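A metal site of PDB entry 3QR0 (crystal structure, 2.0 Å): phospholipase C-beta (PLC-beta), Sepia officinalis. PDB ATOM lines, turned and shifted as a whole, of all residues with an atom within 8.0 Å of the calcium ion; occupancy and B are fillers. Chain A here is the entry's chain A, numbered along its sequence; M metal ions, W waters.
The side-chain carboxylate (OE2) of Glu 417 is in hydrogen-bond range of the side-chain hydroxyl (OG1) of Thr 503 (2.5 Å).
The side-chain amide nitrogen (ND2) of Asn 339 is in hydrogen-bond range of the side-chain amide oxygen (OE1) of Gln 346 (3.1 Å).
O of Asp 370 is in hydrogen-bond range of N of Thr 382 (3.3 Å).
OE1 of Glu 368 is in salt-bridge range of NH2 of Arg 570 (2.9 Å).
The side-chain carboxylate (OE2) of Glu 417 lies within hydrogen-bond range of the backbone NH (N) of Ala 504 (3.3 Å).
The side-chain carboxylate (OE2) of Glu 417 sits at hydrogen-bond distance from a ring nitrogen (NE2) of His 419 (2.7 Å).
OD2 of Asp 370 lies close to OH of Tyr 341 (2.5 Å).
The backbone NH (N) of Cys 371 lies within hydrogen-bond range of the backbone carbonyl oxygen (O) of Glu 417 (2.9 Å).
Of the 26 residues printed, 4 come within 4 Å of the calcium ion.
The calcium ion is bound by OD1 of Asn 339 (2.3 Å), OE2 of Glu 368 (2.4 Å), OE1 of Glu 417 (2.4 Å), water W2 (2.4 Å), water W1 (2.5 Å), OD2 of Asp 370 (2.5 Å) and OD1 of Asp 370 (2.6 Å).
The calcium ion has seven donor atoms within binding distance.
Water W1 lies within hydrogen-bond range of OG1 of Thr 503 (3.0 Å), ND2 of Asn 339 (3.2 Å) and NE2 of His 383 (3.5 Å).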
ATOM      1  N   HIS A 338      -9.575   0.357  -5.756  1.00  0.00           N
ATOM      2  CA  HIS A 338      -9.965  -0.829  -6.545  1.00  0.00           C
ATOM      3  C   HIS A 338     -11.320  -1.410  -6.072  1.00  0.00           C
ATOM      4  O   HIS A 338     -11.588  -1.425  -4.868  1.00  0.00           O
ATOM      5  CB  HIS A 338      -8.887  -1.922  -6.400  1.00  0.00           C
ATOM      6  CG  HIS A 338      -9.298  -3.245  -6.997  1.00  0.00           C
ATOM      7  ND1 HIS A 338      -9.539  -4.362  -6.225  1.00  0.00           N
ATOM      8  CD2 HIS A 338      -9.503  -3.614  -8.270  1.00  0.00           C
ATOM      9  CE1 HIS A 338      -9.877  -5.370  -7.009  1.00  0.00           C
ATOM     10  NE2 HIS A 338      -9.865  -4.937  -8.261  1.00  0.00           N
ATOM     11  N   ASN A 339     -12.103  -1.936  -7.020  1.00  0.00           N
ATOM     12  CA  ASN A 339     -13.466  -2.484  -6.765  1.00  0.00           C
ATOM     13  C   ASN A 339     -14.107  -1.742  -5.589  1.00  0.00           C
ATOM     14  O   ASN A 339     -14.417  -2.323  -4.541  1.00  0.00           O
ATOM     15  CB  ASN A 339     -13.449  -4.013  -6.511  1.00  0.00           C
ATOM     16  CG  ASN A 339     -13.342  -4.851  -7.802  1.00  0.00           C
ATOM     17  OD1 ASN A 339     -13.398  -4.317  -8.912  1.00  0.00           O
ATOM     18  ND2 ASN A 339     -13.199  -6.162  -7.644  1.00  0.00           N
ATOM     19  N   THR A 340     -14.290  -0.457  -5.808  1.00  0.00           N
ATOM     20  CA  THR A 340     -14.652   0.516  -4.778  1.00  0.00           C
ATOM     21  C   THR A 340     -15.965   0.170  -4.088  1.00  0.00           C
ATOM     22  O   THR A 340     -16.134   0.425  -2.891  1.00  0.00           O
ATOM     23  CB  THR A 340     -14.767   1.917  -5.417  1.00  0.00           C
ATOM     24  OG1 THR A 340     -13.601   2.175  -6.206  1.00  0.00           O
ATOM     25  CG2 THR A 340     -14.932   2.997  -4.340  1.00  0.00           C
ATOM     26  N   TYR A 341     -16.884  -0.411  -4.856  1.00  0.00           N
ATOM     27  CA  TYR A 341     -18.202  -0.845  -4.360  1.00  0.00           C
ATOM     28  C   TYR A 341     -18.167  -1.882  -3.227  1.00  0.00           C
ATOM     29  O   TYR A 341     -19.131  -1.987  -2.480  1.00  0.00           O
ATOM     30  CB  TYR A 341     -19.069  -1.365  -5.531  1.00  0.00           C
ATOM     31  CG  TYR A 341     -18.444  -2.519  -6.299  1.00  0.00           C
ATOM     32  CD1 TYR A 341     -18.724  -3.833  -5.966  1.00  0.00           C
ATOM     33  CD2 TYR A 341     -17.565  -2.279  -7.364  1.00  0.00           C
ATOM     34  CE1 TYR A 341     -18.154  -4.890  -6.648  1.00  0.00           C
ATOM     35  CE2 TYR A 341     -16.989  -3.327  -8.045  1.00  0.00           C
ATOM     36  CZ  TYR A 341     -17.292  -4.638  -7.691  1.00  0.00           C
ATOM     37  OH  TYR A 341     -16.722  -5.683  -8.365  1.00  0.00           O
ATOM     38  N   LEU A 342     -17.078  -2.633  -3.099  1.00  0.00           N
ATOM     39  CA  LEU A 342     -16.977  -3.695  -2.094  1.00  0.00           C
ATOM     40  C   LEU A 342     -16.544  -3.160  -0.725  1.00  0.00           C
ATOM     41  O   LEU A 342     -15.563  -2.416  -0.615  1.00  0.00           O
ATOM     42  CB  LEU A 342     -16.023  -4.791  -2.558  1.00  0.00           C
ATOM     43  CG  LEU A 342     -16.469  -5.551  -3.807  1.00  0.00           C
ATOM     44  CD1 LEU A 342     -15.380  -6.525  -4.268  1.00  0.00           C
ATOM     45  CD2 LEU A 342     -17.790  -6.284  -3.574  1.00  0.00           C
ATOM     46  N   GLN A 346     -13.988 -10.135  -1.350  1.00  0.00           N
ATOM     47  CA  GLN A 346     -14.228 -10.041  -2.794  1.00  0.00           C
ATOM     48  C   GLN A 346     -15.301 -10.993  -3.325  1.00  0.00           C
ATOM     49  O   GLN A 346     -15.902 -10.723  -4.376  1.00  0.00           O
ATOM     50  CB  GLN A 346     -12.933 -10.300  -3.584  1.00  0.00           C
ATOM     51  CG  GLN A 346     -11.806  -9.290  -3.344  1.00  0.00           C
ATOM     52  CD  GLN A 346     -12.117  -7.921  -3.915  1.00  0.00           C
ATOM     53  OE1 GLN A 346     -12.345  -7.779  -5.112  1.00  0.00           O
ATOM     54  NE2 GLN A 346     -12.094  -6.913  -3.065  1.00  0.00           N
ATOM     55  N   GLU A 368     -13.531   2.654  -9.093  1.00  0.00           N
ATOM     56  CA  GLU A 368     -13.919   1.600 -10.019  1.00  0.00           C
ATOM     57  C   GLU A 368     -15.392   1.249  -9.899  1.00  0.00           C
ATOM     58  O   GLU A 368     -15.934   1.146  -8.800  1.00  0.00           O
ATOM     59  CB  GLU A 368     -13.067   0.367  -9.776  1.00  0.00           C
ATOM     60  CG  GLU A 368     -13.277  -0.754 -10.801  1.00  0.00           C
ATOM     61  CD  GLU A 368     -12.244  -1.845 -10.693  1.00  0.00           C
ATOM     62  OE1 GLU A 368     -11.408  -1.771  -9.771  1.00  0.00           O
ATOM     63  OE2 GLU A 368     -12.275  -2.773 -11.521  1.00  0.00           O
ATOM     64  N   LEU A 369     -16.035   1.087 -11.049  1.00  0.00           N
ATOM     65  CA  LEU A 369     -17.440   0.696 -11.142  1.00  0.00           C
ATOM     66  C   LEU A 369     -17.513  -0.508 -12.070  1.00  0.00           C
ATOM     67  O   LEU A 369     -17.234  -0.399 -13.271  1.00  0.00           O
ATOM     68  CB  LEU A 369     -18.286   1.849 -11.699  1.00  0.00           C
ATOM     69  CG  LEU A 369     -18.464   3.139 -10.879  1.00  0.00           C
ATOM     70  CD1 LEU A 369     -17.177   3.959 -10.757  1.00  0.00           C
ATOM     71  CD2 LEU A 369     -19.557   4.009 -11.501  1.00  0.00           C
ATOM     72  N   ASP A 370     -17.860  -1.667 -11.512  1.00  0.00           N
ATOM     73  CA  ASP A 370     -18.063  -2.904 -12.277  1.00  0.00           C
ATOM     74  C   ASP A 370     -19.532  -2.989 -12.650  1.00  0.00           C
ATOM     75  O   ASP A 370     -20.375  -3.322 -11.798  1.00  0.00           O
ATOM     76  CB  ASP A 370     -17.688  -4.137 -11.448  1.00  0.00           C
ATOM     77  CG  ASP A 370     -16.201  -4.303 -11.248  1.00  0.00           C
ATOM     78  OD1 ASP A 370     -15.409  -3.401 -11.593  1.00  0.00           O
ATOM     79  OD2 ASP A 370     -15.794  -5.358 -10.707  1.00  0.00           O
ATOM     80  N   CYS A 371     -19.836  -2.724 -13.916  1.00  0.00           N
ATOM     81  CA  CYS A 371     -21.225  -2.593 -14.364  1.00  0.00           C
ATOM     82  C   CYS A 371     -21.735  -3.878 -15.033  1.00  0.00           C
ATOM     83  O   CYS A 371     -21.090  -4.412 -15.939  1.00  0.00           O
ATOM     84  CB  CYS A 371     -21.350  -1.415 -15.324  1.00  0.00           C
ATOM     85  SG  CYS A 371     -20.674   0.121 -14.639  1.00  0.00           S
ATOM     86  N   TRP A 372     -22.891  -4.346 -14.583  1.00  0.00           N
ATOM     87  CA  TRP A 372     -23.534  -5.553 -15.122  1.00  0.00           C
ATOM     88  C   TRP A 372     -25.012  -5.292 -15.419  1.00  0.00           C
ATOM     89  O   TRP A 372     -25.615  -4.361 -14.864  1.00  0.00           O
ATOM     90  CB  TRP A 372     -23.404  -6.714 -14.126  1.00  0.00           C
ATOM     91  CG  TRP A 372     -21.974  -7.093 -13.820  1.00  0.00           C
ATOM     92  CD1 TRP A 372     -21.146  -6.508 -12.907  1.00  0.00           C
ATOM     93  CD2 TRP A 372     -21.202  -8.138 -14.443  1.00  0.00           C
ATOM     94  NE1 TRP A 372     -19.917  -7.123 -12.916  1.00  0.00           N
ATOM     95  CE2 TRP A 372     -19.925  -8.120 -13.857  1.00  0.00           C
ATOM     96  CE3 TRP A 372     -21.484  -9.089 -15.433  1.00  0.00           C
ATOM     97  CZ2 TRP A 372     -18.915  -9.015 -14.229  1.00  0.00           C
ATOM     98  CZ3 TRP A 372     -20.473  -9.971 -15.811  1.00  0.00           C
ATOM     99  CH2 TRP A 372     -19.212  -9.929 -15.209  1.00  0.00           C
ATOM    100  N   THR A 382     -21.667  -4.771  -9.165  1.00  0.00           N
ATOM    101  CA  THR A 382     -21.374  -5.926  -8.332  1.00  0.00           C
ATOM    102  C   THR A 382     -20.104  -6.614  -8.837  1.00  0.00           C
ATOM    103  O   THR A 382     -19.588  -6.261  -9.906  1.00  0.00           O
ATOM    104  CB  THR A 382     -22.550  -6.941  -8.320  1.00  0.00           C
ATOM    105  OG1 THR A 382     -22.352  -7.906  -7.273  1.00  0.00           O
ATOM    106  CG2 THR A 382     -22.679  -7.674  -9.660  1.00  0.00           C
ATOM    107  N   HIS A 383     -19.612  -7.584  -8.078  1.00  0.00           N
ATOM    108  CA  HIS A 383     -18.504  -8.421  -8.526  1.00  0.00           C
ATOM    109  C   HIS A 383     -19.107  -9.640  -9.221  1.00  0.00           C
ATOM    110  O   HIS A 383     -19.694 -10.514  -8.574  1.00  0.00           O
ATOM    111  CB  HIS A 383     -17.597  -8.835  -7.363  1.00  0.00           C
ATOM    112  CG  HIS A 383     -16.255  -9.346  -7.792  1.00  0.00           C
ATOM    113  ND1 HIS A 383     -15.360  -9.922  -6.901  1.00  0.00           N
ATOM    114  CD2 HIS A 383     -15.642  -9.376  -9.000  1.00  0.00           C
ATOM    115  CE1 HIS A 383     -14.267 -10.281  -7.553  1.00  0.00           C
ATOM    116  NE2 HIS A 383     -14.412  -9.963  -8.829  1.00  0.00           N
ATOM    117  N   GLY A 384     -18.984  -9.686 -10.549  1.00  0.00           N
ATOM    118  CA  GLY A 384     -19.613 -10.730 -11.342  1.00  0.00           C
ATOM    119  C   GLY A 384     -19.205 -12.148 -10.999  1.00  0.00           C
ATOM    120  O   GLY A 384     -18.040 -12.395 -10.656  1.00  0.00           O
ATOM    121  N   SER A 415     -13.078   4.417 -13.336  1.00  0.00           N
ATOM    122  CA  SER A 415     -12.676   3.233 -14.087  1.00  0.00           C
ATOM    123  C   SER A 415     -13.887   2.316 -14.222  1.00  0.00           C
ATOM    124  O   SER A 415     -14.319   1.688 -13.247  1.00  0.00           O
ATOM    125  CB  SER A 415     -11.524   2.522 -13.362  1.00  0.00           C
ATOM    126  OG  SER A 415     -11.141   1.346 -14.049  1.00  0.00           O
ATOM    127  N   PHE A 416     -14.439   2.271 -15.443  1.00  0.00           N
ATOM    128  CA  PHE A 416     -15.560   1.396 -15.763  1.00  0.00           C
ATOM    129  C   PHE A 416     -15.046   0.033 -16.220  1.00  0.00           C
ATOM    130  O   PHE A 416     -14.262  -0.066 -17.158  1.00  0.00           O
ATOM    131  CB  PHE A 416     -16.422   2.000 -16.877  1.00  0.00           C
ATOM    132  CG  PHE A 416     -17.402   3.040 -16.405  1.00  0.00           C
ATOM    133  CD1 PHE A 416     -18.767   2.873 -16.597  1.00  0.00           C
ATOM    134  CD2 PHE A 416     -16.964   4.192 -15.766  1.00  0.00           C
ATOM    135  CE1 PHE A 416     -19.676   3.834 -16.165  1.00  0.00           C
ATOM    136  CE2 PHE A 416     -17.861   5.156 -15.327  1.00  0.00           C
ATOM    137  CZ  PHE A 416     -19.220   4.986 -15.525  1.00  0.00           C
ATOM    138  N   GLU A 417     -15.494  -1.021 -15.550  1.00  0.00           N
ATOM    139  CA  GLU A 417     -15.354  -2.372 -16.063  1.00  0.00           C
ATOM    140  C   GLU A 417     -16.748  -2.721 -16.558  1.00  0.00           C
ATOM    141  O   GLU A 417     -17.645  -3.027 -15.777  1.00  0.00           O
ATOM    142  CB  GLU A 417     -14.884  -3.329 -14.970  1.00  0.00           C
ATOM    143  CG  GLU A 417     -14.418  -4.658 -15.483  1.00  0.00           C
ATOM    144  CD  GLU A 417     -14.213  -5.663 -14.369  1.00  0.00           C
ATOM    145  OE1 GLU A 417     -13.427  -5.381 -13.443  1.00  0.00           O
ATOM    146  OE2 GLU A 417     -14.863  -6.733 -14.419  1.00  0.00           O
ATOM    147  N   ASN A 418     -16.924  -2.644 -17.872  1.00  0.00           N
ATOM    148  CA  ASN A 418     -18.239  -2.628 -18.492  1.00  0.00           C
ATOM    149  C   ASN A 418     -18.650  -3.998 -19.023  1.00  0.00           C
ATOM    150  O   ASN A 418     -18.032  -4.521 -19.943  1.00  0.00           O
ATOM    151  CB  ASN A 418     -18.205  -1.595 -19.622  1.00  0.00           C
ATOM    152  CG  ASN A 418     -19.574  -1.124 -20.037  1.00  0.00           C
ATOM    153  OD1 ASN A 418     -20.579  -1.800 -19.815  1.00  0.00           O
ATOM    154  ND2 ASN A 418     -19.618   0.048 -20.653  1.00  0.00           N
ATOM    155  N   HIS A 419     -19.701  -4.579 -18.445  1.00  0.00           N
ATOM    156  CA  HIS A 419     -20.224  -5.866 -18.915  1.00  0.00           C
ATOM    157  C   HIS A 419     -21.653  -5.760 -19.424  1.00  0.00           C
ATOM    158  O   HIS A 419     -22.311  -6.775 -19.647  1.00  0.00           O
ATOM    159  CB  HIS A 419     -20.136  -6.904 -17.809  1.00  0.00           C
ATOM    160  CG  HIS A 419     -18.754  -7.092 -17.281  1.00  0.00           C
ATOM    161  ND1 HIS A 419     -17.858  -7.973 -17.848  1.00  0.00           N
ATOM    162  CD2 HIS A 419     -18.103  -6.495 -16.253  1.00  0.00           C
ATOM    163  CE1 HIS A 419     -16.713  -7.909 -17.185  1.00  0.00           C
ATOM    164  NE2 HIS A 419     -16.835  -7.031 -16.218  1.00  0.00           N
ATOM    165  N   ALA A 501      -6.569 -11.423 -13.758  1.00  0.00           N
ATOM    166  CA  ALA A 501      -7.401 -10.236 -13.963  1.00  0.00           C
ATOM    167  C   ALA A 501      -8.873 -10.448 -13.623  1.00  0.00           C
ATOM    168  O   ALA A 501      -9.607  -9.485 -13.397  1.00  0.00           O
ATOM    169  CB  ALA A 501      -7.275  -9.753 -15.412  1.00  0.00           C
ATOM    170  N   GLY A 502      -9.307 -11.704 -13.582  1.00  0.00           N
ATOM    171  CA  GLY A 502     -10.668 -12.040 -13.171  1.00  0.00           C
ATOM    172  C   GLY A 502     -11.671 -11.505 -14.169  1.00  0.00           C
ATOM    173  O   GLY A 502     -11.469 -11.617 -15.373  1.00  0.00           O
ATOM    174  N   THR A 503     -12.738 -10.891 -13.656  1.00  0.00           N
ATOM    175  CA  THR A 503     -13.785 -10.349 -14.528  1.00  0.00           C
ATOM    176  C   THR A 503     -13.290  -9.225 -15.446  1.00  0.00           C
ATOM    177  O   THR A 503     -13.881  -8.965 -16.483  1.00  0.00           O
ATOM    178  CB  THR A 503     -15.008  -9.841 -13.725  1.00  0.00           C
ATOM    179  OG1 THR A 503     -14.620  -8.750 -12.888  1.00  0.00           O
ATOM    180  CG2 THR A 503     -15.623 -10.963 -12.875  1.00  0.00           C
ATOM    181  N   ALA A 504     -12.207  -8.559 -15.062  1.00  0.00           N
ATOM    182  CA  ALA A 504     -11.637  -7.481 -15.882  1.00  0.00           C
ATOM    183  C   ALA A 504     -10.993  -7.977 -17.183  1.00  0.00           C
ATOM    184  O   ALA A 504     -10.709  -7.175 -18.076  1.00  0.00           O
ATOM    185  CB  ALA A 504     -10.624  -6.684 -15.069  1.00  0.00           C
ATOM    186  N   ARG A 570      -2.531   2.303 -14.736  1.00  0.00           N
ATOM    187  CA  ARG A 570      -3.296   1.918 -13.560  1.00  0.00           C
ATOM    188  C   ARG A 570      -2.924   0.488 -13.197  1.00  0.00           C
ATOM    189  O   ARG A 570      -2.751  -0.354 -14.074  1.00  0.00           O
ATOM    190  CB  ARG A 570      -4.801   2.031 -13.844  1.00  0.00           C
ATOM    191  CG  ARG A 570      -5.696   1.599 -12.691  1.00  0.00           C
ATOM    192  CD  ARG A 570      -7.155   1.994 -12.946  1.00  0.00           C
ATOM    193  NE  ARG A 570      -8.012   1.576 -11.840  1.00  0.00           N
ATOM    194  CZ  ARG A 570      -8.546   0.361 -11.693  1.00  0.00           C
ATOM    195  NH1 ARG A 570      -8.338  -0.595 -12.593  1.00  0.00           N
ATOM    196  NH2 ARG A 570      -9.304   0.102 -10.632  1.00  0.00           N
ATOM    197  N   TYR A 572      -3.989  -2.830 -10.506  1.00  0.00           N
ATOM    198  CA  TYR A 572      -4.996  -3.338  -9.571  1.00  0.00           C
ATOM    199  C   TYR A 572      -4.668  -4.759  -9.096  1.00  0.00           C
ATOM    200  O   TYR A 572      -3.980  -5.509  -9.801  1.00  0.00           O
ATOM    201  CB  TYR A 572      -6.405  -3.236 -10.172  1.00  0.00           C
ATOM    202  CG  TYR A 572      -6.605  -4.052 -11.416  1.00  0.00           C
ATOM    203  CD1 TYR A 572      -7.101  -5.352 -11.347  1.00  0.00           C
ATOM    204  CD2 TYR A 572      -6.321  -3.526 -12.677  1.00  0.00           C
ATOM    205  CE1 TYR A 572      -7.301  -6.104 -12.485  1.00  0.00           C
ATOM    206  CE2 TYR A 572      -6.514  -4.281 -13.837  1.00  0.00           C
ATOM    207  CZ  TYR A 572      -7.004  -5.565 -13.730  1.00  0.00           C
ATOM    208  OH  TYR A 572      -7.212  -6.339 -14.850  1.00  0.00           O
ATOM    209  N   PRO A 573      -5.149  -5.120  -7.884  1.00  0.00           N
ATOM    210  CA  PRO A 573      -4.758  -6.411  -7.316  1.00  0.00           C
ATOM    211  C   PRO A 573      -5.288  -7.615  -8.085  1.00  0.00           C
ATOM    212  O   PRO A 573      -6.377  -7.569  -8.650  1.00  0.00           O
ATOM    213  CB  PRO A 573      -5.347  -6.363  -5.892  1.00  0.00           C
ATOM    214  CG  PRO A 573      -6.343  -5.275  -5.899  1.00  0.00           C
ATOM    215  CD  PRO A 573      -5.904  -4.296  -6.940  1.00  0.00           C
HETATM  216 CA    CA M   1     -13.351  -4.847 -11.129  1.00  0.00          CA
HETATM  217  O   HOH W   1     -13.206  -7.254 -10.677  1.00  0.00           O
HETATM  218  O   HOH W   2     -11.066  -5.576 -10.745  1.00  0.00           O
